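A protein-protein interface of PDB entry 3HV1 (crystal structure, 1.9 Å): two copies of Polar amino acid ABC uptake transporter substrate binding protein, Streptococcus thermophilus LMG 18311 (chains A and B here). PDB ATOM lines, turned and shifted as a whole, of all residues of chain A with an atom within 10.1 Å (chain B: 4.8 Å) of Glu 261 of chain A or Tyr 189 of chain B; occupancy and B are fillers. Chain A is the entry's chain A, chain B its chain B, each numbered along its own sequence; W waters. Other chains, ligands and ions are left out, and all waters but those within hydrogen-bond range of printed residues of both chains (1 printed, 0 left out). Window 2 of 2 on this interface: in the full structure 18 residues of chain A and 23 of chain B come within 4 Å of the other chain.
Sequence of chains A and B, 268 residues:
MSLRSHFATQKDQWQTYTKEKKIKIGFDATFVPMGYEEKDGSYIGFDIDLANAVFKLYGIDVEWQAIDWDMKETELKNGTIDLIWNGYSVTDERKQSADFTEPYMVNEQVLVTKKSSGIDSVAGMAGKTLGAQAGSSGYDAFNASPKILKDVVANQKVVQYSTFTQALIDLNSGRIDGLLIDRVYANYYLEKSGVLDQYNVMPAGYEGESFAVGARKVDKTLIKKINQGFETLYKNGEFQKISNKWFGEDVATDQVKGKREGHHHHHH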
ATOM      1  N   GLU A 102      -6.491  36.438  26.717  1.00  0.00           N
ATOM      2  CA  GLU A 102      -5.072  36.306  26.430  1.00  0.00           C
ATOM      3  C   GLU A 102      -4.527  37.729  26.556  1.00  0.00           C
ATOM      4  O   GLU A 102      -5.292  38.692  26.488  1.00  0.00           O
ATOM      5  CB  GLU A 102      -4.876  35.808  24.995  1.00  0.00           C
ATOM      6  CG  GLU A 102      -5.385  34.404  24.763  1.00  0.00           C
ATOM      7  CD  GLU A 102      -4.789  33.420  25.744  1.00  0.00           C
ATOM      8  OE1 GLU A 102      -3.554  33.465  25.939  1.00  0.00           O
ATOM      9  OE2 GLU A 102      -5.549  32.602  26.317  1.00  0.00           O
ATOM     10  N   ASP A 254       2.203  37.950  20.731  1.00  0.00           N
ATOM     11  CA  ASP A 254       2.117  36.852  19.785  1.00  0.00           C
ATOM     12  C   ASP A 254       0.707  36.249  19.782  1.00  0.00           C
ATOM     13  O   ASP A 254       0.224  35.810  18.743  1.00  0.00           O
ATOM     14  CB  ASP A 254       3.162  35.786  20.117  1.00  0.00           C
ATOM     15  CG  ASP A 254       4.571  36.235  19.777  1.00  0.00           C
ATOM     16  OD1 ASP A 254       4.726  37.044  18.836  1.00  0.00           O
ATOM     17  OD2 ASP A 254       5.523  35.771  20.431  1.00  0.00           O
ATOM     18  N   GLN A 255       0.040  36.240  20.935  1.00  0.00           N
ATOM     19  CA  GLN A 255      -1.317  35.698  21.000  1.00  0.00           C
ATOM     20  C   GLN A 255      -2.271  36.489  20.103  1.00  0.00           C
ATOM     21  O   GLN A 255      -3.073  35.902  19.364  1.00  0.00           O
ATOM     22  CB  GLN A 255      -1.840  35.694  22.443  1.00  0.00           C
ATOM     23  CG  GLN A 255      -1.150  34.668  23.335  1.00  0.00           C
ATOM     24  CD  GLN A 255      -0.043  35.266  24.164  1.00  0.00           C
ATOM     25  OE1 GLN A 255       0.635  36.205  23.739  1.00  0.00           O
ATOM     26  NE2 GLN A 255       0.161  34.718  25.355  1.00  0.00           N
ATOM     27  N   VAL A 256      -2.189  37.816  20.170  1.00  0.00           N
ATOM     28  CA  VAL A 256      -3.038  38.670  19.343  1.00  0.00           C
ATOM     29  C   VAL A 256      -2.747  38.388  17.868  1.00  0.00           C
ATOM     30  O   VAL A 256      -3.640  38.472  17.025  1.00  0.00           O
ATOM     31  CB  VAL A 256      -2.783  40.174  19.645  1.00  0.00           C
ATOM     32  CG1 VAL A 256      -3.327  41.048  18.530  1.00  0.00           C
ATOM     33  CG2 VAL A 256      -3.444  40.543  20.957  1.00  0.00           C
ATOM     34  N   LYS A 257      -1.494  38.048  17.571  1.00  0.00           N
ATOM     35  CA  LYS A 257      -1.070  37.755  16.205  1.00  0.00           C
ATOM     36  C   LYS A 257      -1.488  36.362  15.731  1.00  0.00           C
ATOM     37  O   LYS A 257      -1.270  36.006  14.576  1.00  0.00           O
ATOM     38  CB  LYS A 257       0.448  37.896  16.084  1.00  0.00           C
ATOM     39  CG  LYS A 257       0.964  39.306  16.263  1.00  0.00           C
ATOM     40  CD  LYS A 257       2.476  39.359  16.105  1.00  0.00           C
ATOM     41  CE  LYS A 257       3.006  40.782  16.240  1.00  0.00           C
ATOM     42  NZ  LYS A 257       4.497  40.840  16.151  1.00  0.00           N
ATOM     43  N   GLY A 258      -2.076  35.575  16.623  1.00  0.00           N
ATOM     44  CA  GLY A 258      -2.515  34.239  16.255  1.00  0.00           C
ATOM     45  C   GLY A 258      -1.469  33.144  16.417  1.00  0.00           C
ATOM     46  O   GLY A 258      -1.702  32.002  16.021  1.00  0.00           O
ATOM     47  N   LYS A 259      -0.321  33.488  16.996  1.00  0.00           N
ATOM     48  CA  LYS A 259       0.762  32.529  17.212  1.00  0.00           C
ATOM     49  C   LYS A 259       0.602  31.865  18.579  1.00  0.00           C
ATOM     50  O   LYS A 259       1.050  32.408  19.589  1.00  0.00           O
ATOM     51  CB  LYS A 259       2.112  33.243  17.159  1.00  0.00           C
ATOM     52  CG  LYS A 259       2.367  34.012  15.877  1.00  0.00           C
ATOM     53  CD  LYS A 259       3.675  34.774  15.957  1.00  0.00           C
ATOM     54  CE  LYS A 259       4.029  35.427  14.629  1.00  0.00           C
ATOM     55  NZ  LYS A 259       2.973  36.375  14.166  1.00  0.00           N
ATOM     56  N   ARG A 260      -0.017  30.688  18.611  1.00  0.00           N
ATOM     57  CA  ARG A 260      -0.236  29.994  19.879  1.00  0.00           C
ATOM     58  C   ARG A 260       0.861  28.999  20.254  1.00  0.00           C
ATOM     59  O   ARG A 260       0.819  28.407  21.333  1.00  0.00           O
ATOM     60  CB  ARG A 260      -1.588  29.263  19.868  1.00  0.00           C
ATOM     61  CG  ARG A 260      -2.560  29.674  18.757  1.00  0.00           C
ATOM     62  CD  ARG A 260      -2.963  31.152  18.788  1.00  0.00           C
ATOM     63  NE  ARG A 260      -3.780  31.520  19.946  1.00  0.00           N
ATOM     64  CZ  ARG A 260      -3.292  31.824  21.146  1.00  0.00           C
ATOM     65  NH1 ARG A 260      -1.982  31.812  21.361  1.00  0.00           N
ATOM     66  NH2 ARG A 260      -4.118  32.146  22.135  1.00  0.00           N
ATOM     67  N   GLU A 261       1.844  28.816  19.380  1.00  0.00           N
ATOM     68  CA  GLU A 261       2.922  27.871  19.660  1.00  0.00           C
ATOM     69  C   GLU A 261       3.640  28.157  20.970  1.00  0.00           C
ATOM     70  O   GLU A 261       4.124  29.268  21.194  1.00  0.00           O
ATOM     71  CB  GLU A 261       3.955  27.869  18.535  1.00  0.00           C
ATOM     72  CG  GLU A 261       5.047  26.821  18.735  1.00  0.00           C
ATOM     73  CD  GLU A 261       6.154  26.915  17.705  1.00  0.00           C
ATOM     74  OE1 GLU A 261       5.849  27.213  16.532  1.00  0.00           O
ATOM     75  OE2 GLU A 261       7.326  26.678  18.062  1.00  0.00           O
ATOM     76  N   GLY A 262       3.712  27.139  21.824  1.00  0.00           N
ATOM     77  CA  GLY A 262       4.392  27.273  23.100  1.00  0.00           C
ATOM     78  C   GLY A 262       3.564  27.839  24.237  1.00  0.00           C
ATOM     79  O   GLY A 262       4.081  28.052  25.330  1.00  0.00           O
ATOM     80  N   HIS A 263       2.281  28.077  24.000  1.00  0.00           N
ATOM     81  CA  HIS A 263       1.433  28.637  25.043  1.00  0.00           C
ATOM     82  C   HIS A 263       0.441  27.650  25.655  1.00  0.00           C
ATOM     83  O   HIS A 263      -0.377  28.027  26.494  1.00  0.00           O
ATOM     84  CB  HIS A 263       0.700  29.871  24.508  1.00  0.00           C
ATOM     85  CG  HIS A 263       1.607  31.030  24.232  1.00  0.00           C
ATOM     86  ND1 HIS A 263       2.281  31.699  25.232  1.00  0.00           N
ATOM     87  CD2 HIS A 263       1.977  31.618  23.070  1.00  0.00           C
ATOM     88  CE1 HIS A 263       3.029  32.648  24.697  1.00  0.00           C
ATOM     89  NE2 HIS A 263       2.863  32.620  23.387  1.00  0.00           N
ATOM     90  N   HIS A 264       0.522  26.389  25.242  1.00  0.00           N
ATOM     91  CA  HIS A 264      -0.365  25.366  25.785  1.00  0.00           C
ATOM     92  C   HIS A 264       0.161  24.912  27.154  1.00  0.00           C
ATOM     93  O   HIS A 264       1.350  24.632  27.307  1.00  0.00           O
ATOM     94  CB  HIS A 264      -0.448  24.158  24.841  1.00  0.00           C
ATOM     95  CG  HIS A 264      -0.860  24.501  23.442  1.00  0.00           C
ATOM     96  ND1 HIS A 264      -0.016  25.125  22.548  1.00  0.00           N
ATOM     97  CD2 HIS A 264      -2.029  24.311  22.784  1.00  0.00           C
ATOM     98  CE1 HIS A 264      -0.646  25.305  21.402  1.00  0.00           C
ATOM     99  NE2 HIS A 264      -1.870  24.820  21.518  1.00  0.00           N
ATOM    100  N   HIS A 265      -0.734  24.863  28.140  1.00  0.00           N
ATOM    101  CA  HIS A 265      -0.416  24.445  29.511  1.00  0.00           C
ATOM    102  C   HIS A 265      -1.279  23.231  29.838  1.00  0.00           C
ATOM    103  O   HIS A 265      -2.506  23.320  29.788  1.00  0.00           O
ATOM    104  CB  HIS A 265      -0.729  25.572  30.502  1.00  0.00           C
ATOM    105  CG  HIS A 265      -2.023  26.274  30.226  1.00  0.00           C
ATOM    106  ND1 HIS A 265      -3.156  25.612  29.805  1.00  0.00           N
ATOM    107  CD2 HIS A 265      -2.364  27.582  30.310  1.00  0.00           C
ATOM    108  CE1 HIS A 265      -4.137  26.481  29.636  1.00  0.00           C
ATOM    109  NE2 HIS A 265      -3.683  27.683  29.937  1.00  0.00           N
ATOM    110  N   THR B  30      -2.892  23.410  16.574  1.00  0.00           N
ATOM    111  CA  THR B  30      -1.863  24.368  16.960  1.00  0.00           C
ATOM    112  C   THR B  30      -0.891  23.835  18.005  1.00  0.00           C
ATOM    113  O   THR B  30       0.068  24.520  18.360  1.00  0.00           O
ATOM    114  CB  THR B  30      -2.483  25.630  17.558  1.00  0.00           C
ATOM    115  OG1 THR B  30      -3.027  25.312  18.845  1.00  0.00           O
ATOM    116  CG2 THR B  30      -3.589  26.156  16.666  1.00  0.00           C
ATOM    117  N   VAL B  32       2.053  22.345  19.083  1.00  0.00           N
ATOM    118  CA  VAL B  32       3.413  21.915  18.804  1.00  0.00           C
ATOM    119  C   VAL B  32       3.914  21.383  20.147  1.00  0.00           C
ATOM    120  O   VAL B  32       3.691  22.008  21.183  1.00  0.00           O
ATOM    121  CB  VAL B  32       4.286  23.105  18.369  1.00  0.00           C
ATOM    122  CG1 VAL B  32       5.688  22.627  18.028  1.00  0.00           C
ATOM    123  CG2 VAL B  32       3.646  23.812  17.171  1.00  0.00           C
ATOM    124  N   PHE B 164       9.408  30.183  25.798  1.00  0.00           N
ATOM    125  CA  PHE B 164      10.596  29.402  26.128  1.00  0.00           C
ATOM    126  C   PHE B 164      11.827  29.979  25.442  1.00  0.00           C
ATOM    127  O   PHE B 164      12.934  29.894  25.966  1.00  0.00           O
ATOM    128  CB  PHE B 164      10.408  27.947  25.693  1.00  0.00           C
ATOM    129  CG  PHE B 164      11.592  27.067  25.985  1.00  0.00           C
ATOM    130  CD1 PHE B 164      11.865  26.653  27.286  1.00  0.00           C
ATOM    131  CD2 PHE B 164      12.440  26.657  24.960  1.00  0.00           C
ATOM    132  CE1 PHE B 164      12.965  25.841  27.560  1.00  0.00           C
ATOM    133  CE2 PHE B 164      13.542  25.847  25.224  1.00  0.00           C
ATOM    134  CZ  PHE B 164      13.805  25.438  26.526  1.00  0.00           C
ATOM    135  N   TYR B 185       8.309  20.794  25.993  1.00  0.00           N
ATOM    136  CA  TYR B 185       8.921  21.958  25.349  1.00  0.00           C
ATOM    137  C   TYR B 185      10.448  21.977  25.429  1.00  0.00           C
ATOM    138  O   TYR B 185      11.124  22.242  24.441  1.00  0.00           O
ATOM    139  CB  TYR B 185       8.381  23.266  25.948  1.00  0.00           C
ATOM    140  CG  TYR B 185       6.916  23.547  25.673  1.00  0.00           C
ATOM    141  CD1 TYR B 185       6.343  23.246  24.441  1.00  0.00           C
ATOM    142  CD2 TYR B 185       6.110  24.148  26.642  1.00  0.00           C
ATOM    143  CE1 TYR B 185       4.997  23.537  24.178  1.00  0.00           C
ATOM    144  CE2 TYR B 185       4.767  24.446  26.387  1.00  0.00           C
ATOM    145  CZ  TYR B 185       4.220  24.138  25.155  1.00  0.00           C
ATOM    146  OH  TYR B 185       2.896  24.434  24.901  1.00  0.00           O
ATOM    147  N   ALA B 186      10.989  21.713  26.611  1.00  0.00           N
ATOM    148  CA  ALA B 186      12.433  21.709  26.794  1.00  0.00           C
ATOM    149  C   ALA B 186      13.108  20.767  25.805  1.00  0.00           C
ATOM    150  O   ALA B 186      14.000  21.172  25.056  1.00  0.00           O
ATOM    151  CB  ALA B 186      12.782  21.294  28.220  1.00  0.00           C
ATOM    152  N   ASN B 187      12.676  19.509  25.796  1.00  0.00           N
ATOM    153  CA  ASN B 187      13.278  18.533  24.900  1.00  0.00           C
ATOM    154  C   ASN B 187      13.047  18.808  23.429  1.00  0.00           C
ATOM    155  O   ASN B 187      13.968  18.718  22.638  1.00  0.00           O
ATOM    156  CB  ASN B 187      12.810  17.116  25.240  1.00  0.00           C
ATOM    157  CG  ASN B 187      13.494  16.566  26.473  1.00  0.00           C
ATOM    158  OD1 ASN B 187      13.200  16.976  27.591  1.00  0.00           O
ATOM    159  ND2 ASN B 187      14.426  15.647  26.272  1.00  0.00           N
ATOM    160  N   TYR B 188      11.823  19.145  23.055  1.00  0.00           N
ATOM    161  CA  TYR B 188      11.548  19.418  21.656  1.00  0.00           C
ATOM    162  C   TYR B 188      12.403  20.553  21.105  1.00  0.00           C
ATOM    163  O   TYR B 188      13.068  20.400  20.083  1.00  0.00           O
ATOM    164  CB  TYR B 188      10.077  19.773  21.453  1.00  0.00           C
ATOM    165  CG  TYR B 188       9.785  20.328  20.076  1.00  0.00           C
ATOM    166  CD1 TYR B 188       9.915  19.529  18.937  1.00  0.00           C
ATOM    167  CD2 TYR B 188       9.380  21.655  19.909  1.00  0.00           C
ATOM    168  CE1 TYR B 188       9.645  20.035  17.666  1.00  0.00           C
ATOM    169  CE2 TYR B 188       9.108  22.170  18.639  1.00  0.00           C
ATOM    170  CZ  TYR B 188       9.240  21.352  17.526  1.00  0.00           C
ATOM    171  OH  TYR B 188       8.935  21.847  16.282  1.00  0.00           O
ATOM    172  N   TYR B 189      12.376  21.695  21.779  1.00  0.00           N
ATOM    173  CA  TYR B 189      13.123  22.858  21.322  1.00  0.00           C
ATOM    174  C   TYR B 189      14.635  22.726  21.354  1.00  0.00           C
ATOM    175  O   TYR B 189      15.305  23.084  20.391  1.00  0.00           O
ATOM    176  CB  TYR B 189      12.713  24.089  22.121  1.00  0.00           C
ATOM    177  CG  TYR B 189      11.353  24.593  21.738  1.00  0.00           C
ATOM    178  CD1 TYR B 189      11.088  25.004  20.432  1.00  0.00           C
ATOM    179  CD2 TYR B 189      10.321  24.656  22.673  1.00  0.00           C
ATOM    180  CE1 TYR B 189       9.834  25.465  20.067  1.00  0.00           C
ATOM    181  CE2 TYR B 189       9.059  25.120  22.318  1.00  0.00           C
ATOM    182  CZ  TYR B 189       8.825  25.521  21.014  1.00  0.00           C
ATOM    183  OH  TYR B 189       7.583  25.983  20.659  1.00  0.00           O
ATOM    184  N   LEU B 190      15.171  22.235  22.466  1.00  0.00           N
ATOM    185  CA  LEU B 190      16.613  22.085  22.591  1.00  0.00           C
ATOM    186  C   LEU B 190      17.142  21.042  21.617  1.00  0.00           C
ATOM    187  O   LEU B 190      18.249  21.181  21.099  1.00  0.00           O
ATOM    188  CB  LEU B 190      16.985  21.705  24.024  1.00  0.00           C
ATOM    189  CG  LEU B 190      16.660  22.760  25.086  1.00  0.00           C
ATOM    190  CD1 LEU B 190      17.145  22.291  26.447  1.00  0.00           C
ATOM    191  CD2 LEU B 190      17.333  24.073  24.712  1.00  0.00           C
ATOM    192  N   GLU B 191      16.355  20.001  21.364  1.00  0.00           N
ATOM    193  CA  GLU B 191      16.775  18.957  20.429  1.00  0.00           C
ATOM    194  C   GLU B 191      16.665  19.460  18.990  1.00  0.00           C
ATOM    195  O   GLU B 191      17.514  19.158  18.157  1.00  0.00           O
ATOM    196  CB  GLU B 191      15.921  17.692  20.597  1.00  0.00           C
ATOM    197  CG  GLU B 191      16.140  16.609  19.522  1.00  0.00           C
ATOM    198  CD  GLU B 191      17.530  15.963  19.556  1.00  0.00           C
ATOM    199  OE1 GLU B 191      18.311  16.229  20.495  1.00  0.00           O
ATOM    200  OE2 GLU B 191      17.836  15.173  18.639  1.00  0.00           O
ATOM    201  N   LYS B 192      15.617  20.226  18.702  1.00  0.00           N
ATOM    202  CA  LYS B 192      15.433  20.750  17.356  1.00  0.00           C
ATOM    203  C   LYS B 192      16.566  21.719  17.013  1.00  0.00           C
ATOM    204  O   LYS B 192      16.971  21.827  15.858  1.00  0.00           O
ATOM    205  CB  LYS B 192      14.078  21.449  17.241  1.00  0.00           C
ATOM    206  CG  LYS B 192      13.702  21.865  15.829  1.00  0.00           C
ATOM    207  CD  LYS B 192      12.236  22.261  15.764  1.00  0.00           C
ATOM    208  CE  LYS B 192      11.870  22.842  14.408  1.00  0.00           C
ATOM    209  NZ  LYS B 192      12.530  24.157  14.184  1.00  0.00           N
ATOM    210  N   SER B 193      17.078  22.412  18.028  1.00  0.00           N
ATOM    211  CA  SER B 193      18.172  23.368  17.853  1.00  0.00           C
ATOM    212  C   SER B 193      19.547  22.716  18.009  1.00  0.00           C
ATOM    213  O   SER B 193      20.579  23.389  17.924  1.00  0.00           O
ATOM    214  CB  SER B 193      18.036  24.513  18.859  1.00  0.00           C
ATOM    215  OG  SER B 193      16.968  25.368  18.495  1.00  0.00           O
HETATM  216  O   HOH W   1       2.502  24.453  21.570  1.00  0.00           O
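The side-chain carboxylate of Glu 261 of chain A sits at hydrogen-bond distance from the side-chain hydroxyl of Tyr 189 of chain B, 2.7 Å away. OH of Tyr 185 of chain B sits at hydrogen-bond distance from O of His 264 of chain A (2.9 Å). NE2 of His 264 of chain A is in hydrogen-bond range of OG1 of Thr 30 of chain B, 3.0 Å away.
Glu 261 of chain A touches two residues of chain B. Tyr 189 of chain B touches just one residue of chain A: Glu 261 (2.7 Å). Of chain A, only Glu 261 (3.7 Å) comes within 4 Å of Val 32 of chain B. Of chain A, only Gly 262, His 263 and His 264 come within 4 Å of Tyr 185 of chain B. No residue of chain A comes within 4 Å of Tyr 188 of chain B. No residue of chain A comes within 4 Å of Leu 190 of chain B. No residue of chain A comes within 4 Å of Ser 193 of chain B. Of the printed residues of chain B, Gly 262 of chain A touches Tyr 185. Printed residues of chain B within 4 Å of His 264 of chain A: Thr 30 and Tyr 185. Of the printed residues of chain A, Thr 30 of chain B touches His 264 (3.0 Å). Glu 191 of chain B touches none of the printed residues of chain A. Gly 258 of chain A touches none of the printed residues of chain B.
Among the printed residues, pairs that only touch across the chains: Gly 262 of chain A with Tyr 185 of chain B (3.5 Å), Glu 261 of chain A with Val 32 of chain B (3.7 Å) and His 263 of chain A with Tyr 185 of chain B (3.8 Å).
Water W1 lies within hydrogen-bond range of O of Val 32 of chain B, ND1 of His 264 of chain A, N of Gly 262 of chain A and OH of Tyr 185 of chain B.
Of the 13 printed residues of chain A, 4 touch a printed residue of chain B. Printed residues of chain A that touch a printed residue of chain B: Glu 261, Gly 262, His 263 and His 264. Of the 12 printed residues of chain B, 4 touch a printed residue of chain A. Hydrophobic or aromatic side chains of chain B that line the printed part of chain A: Val 32, Tyr 185 and Tyr 189. Among the printed residues, 6 pairs touch across the chains.
No position is printed for both chains. Of the 6 pairs that touch across the chains among the printed residues, none has its exchanged pair printed and touching as well.
The backbone carbonyl oxygen of Tyr 189 of chain B sits at hydrogen-bond distance from the side-chain hydroxyl of Ser 193 of chain B, 3.4 Å away.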
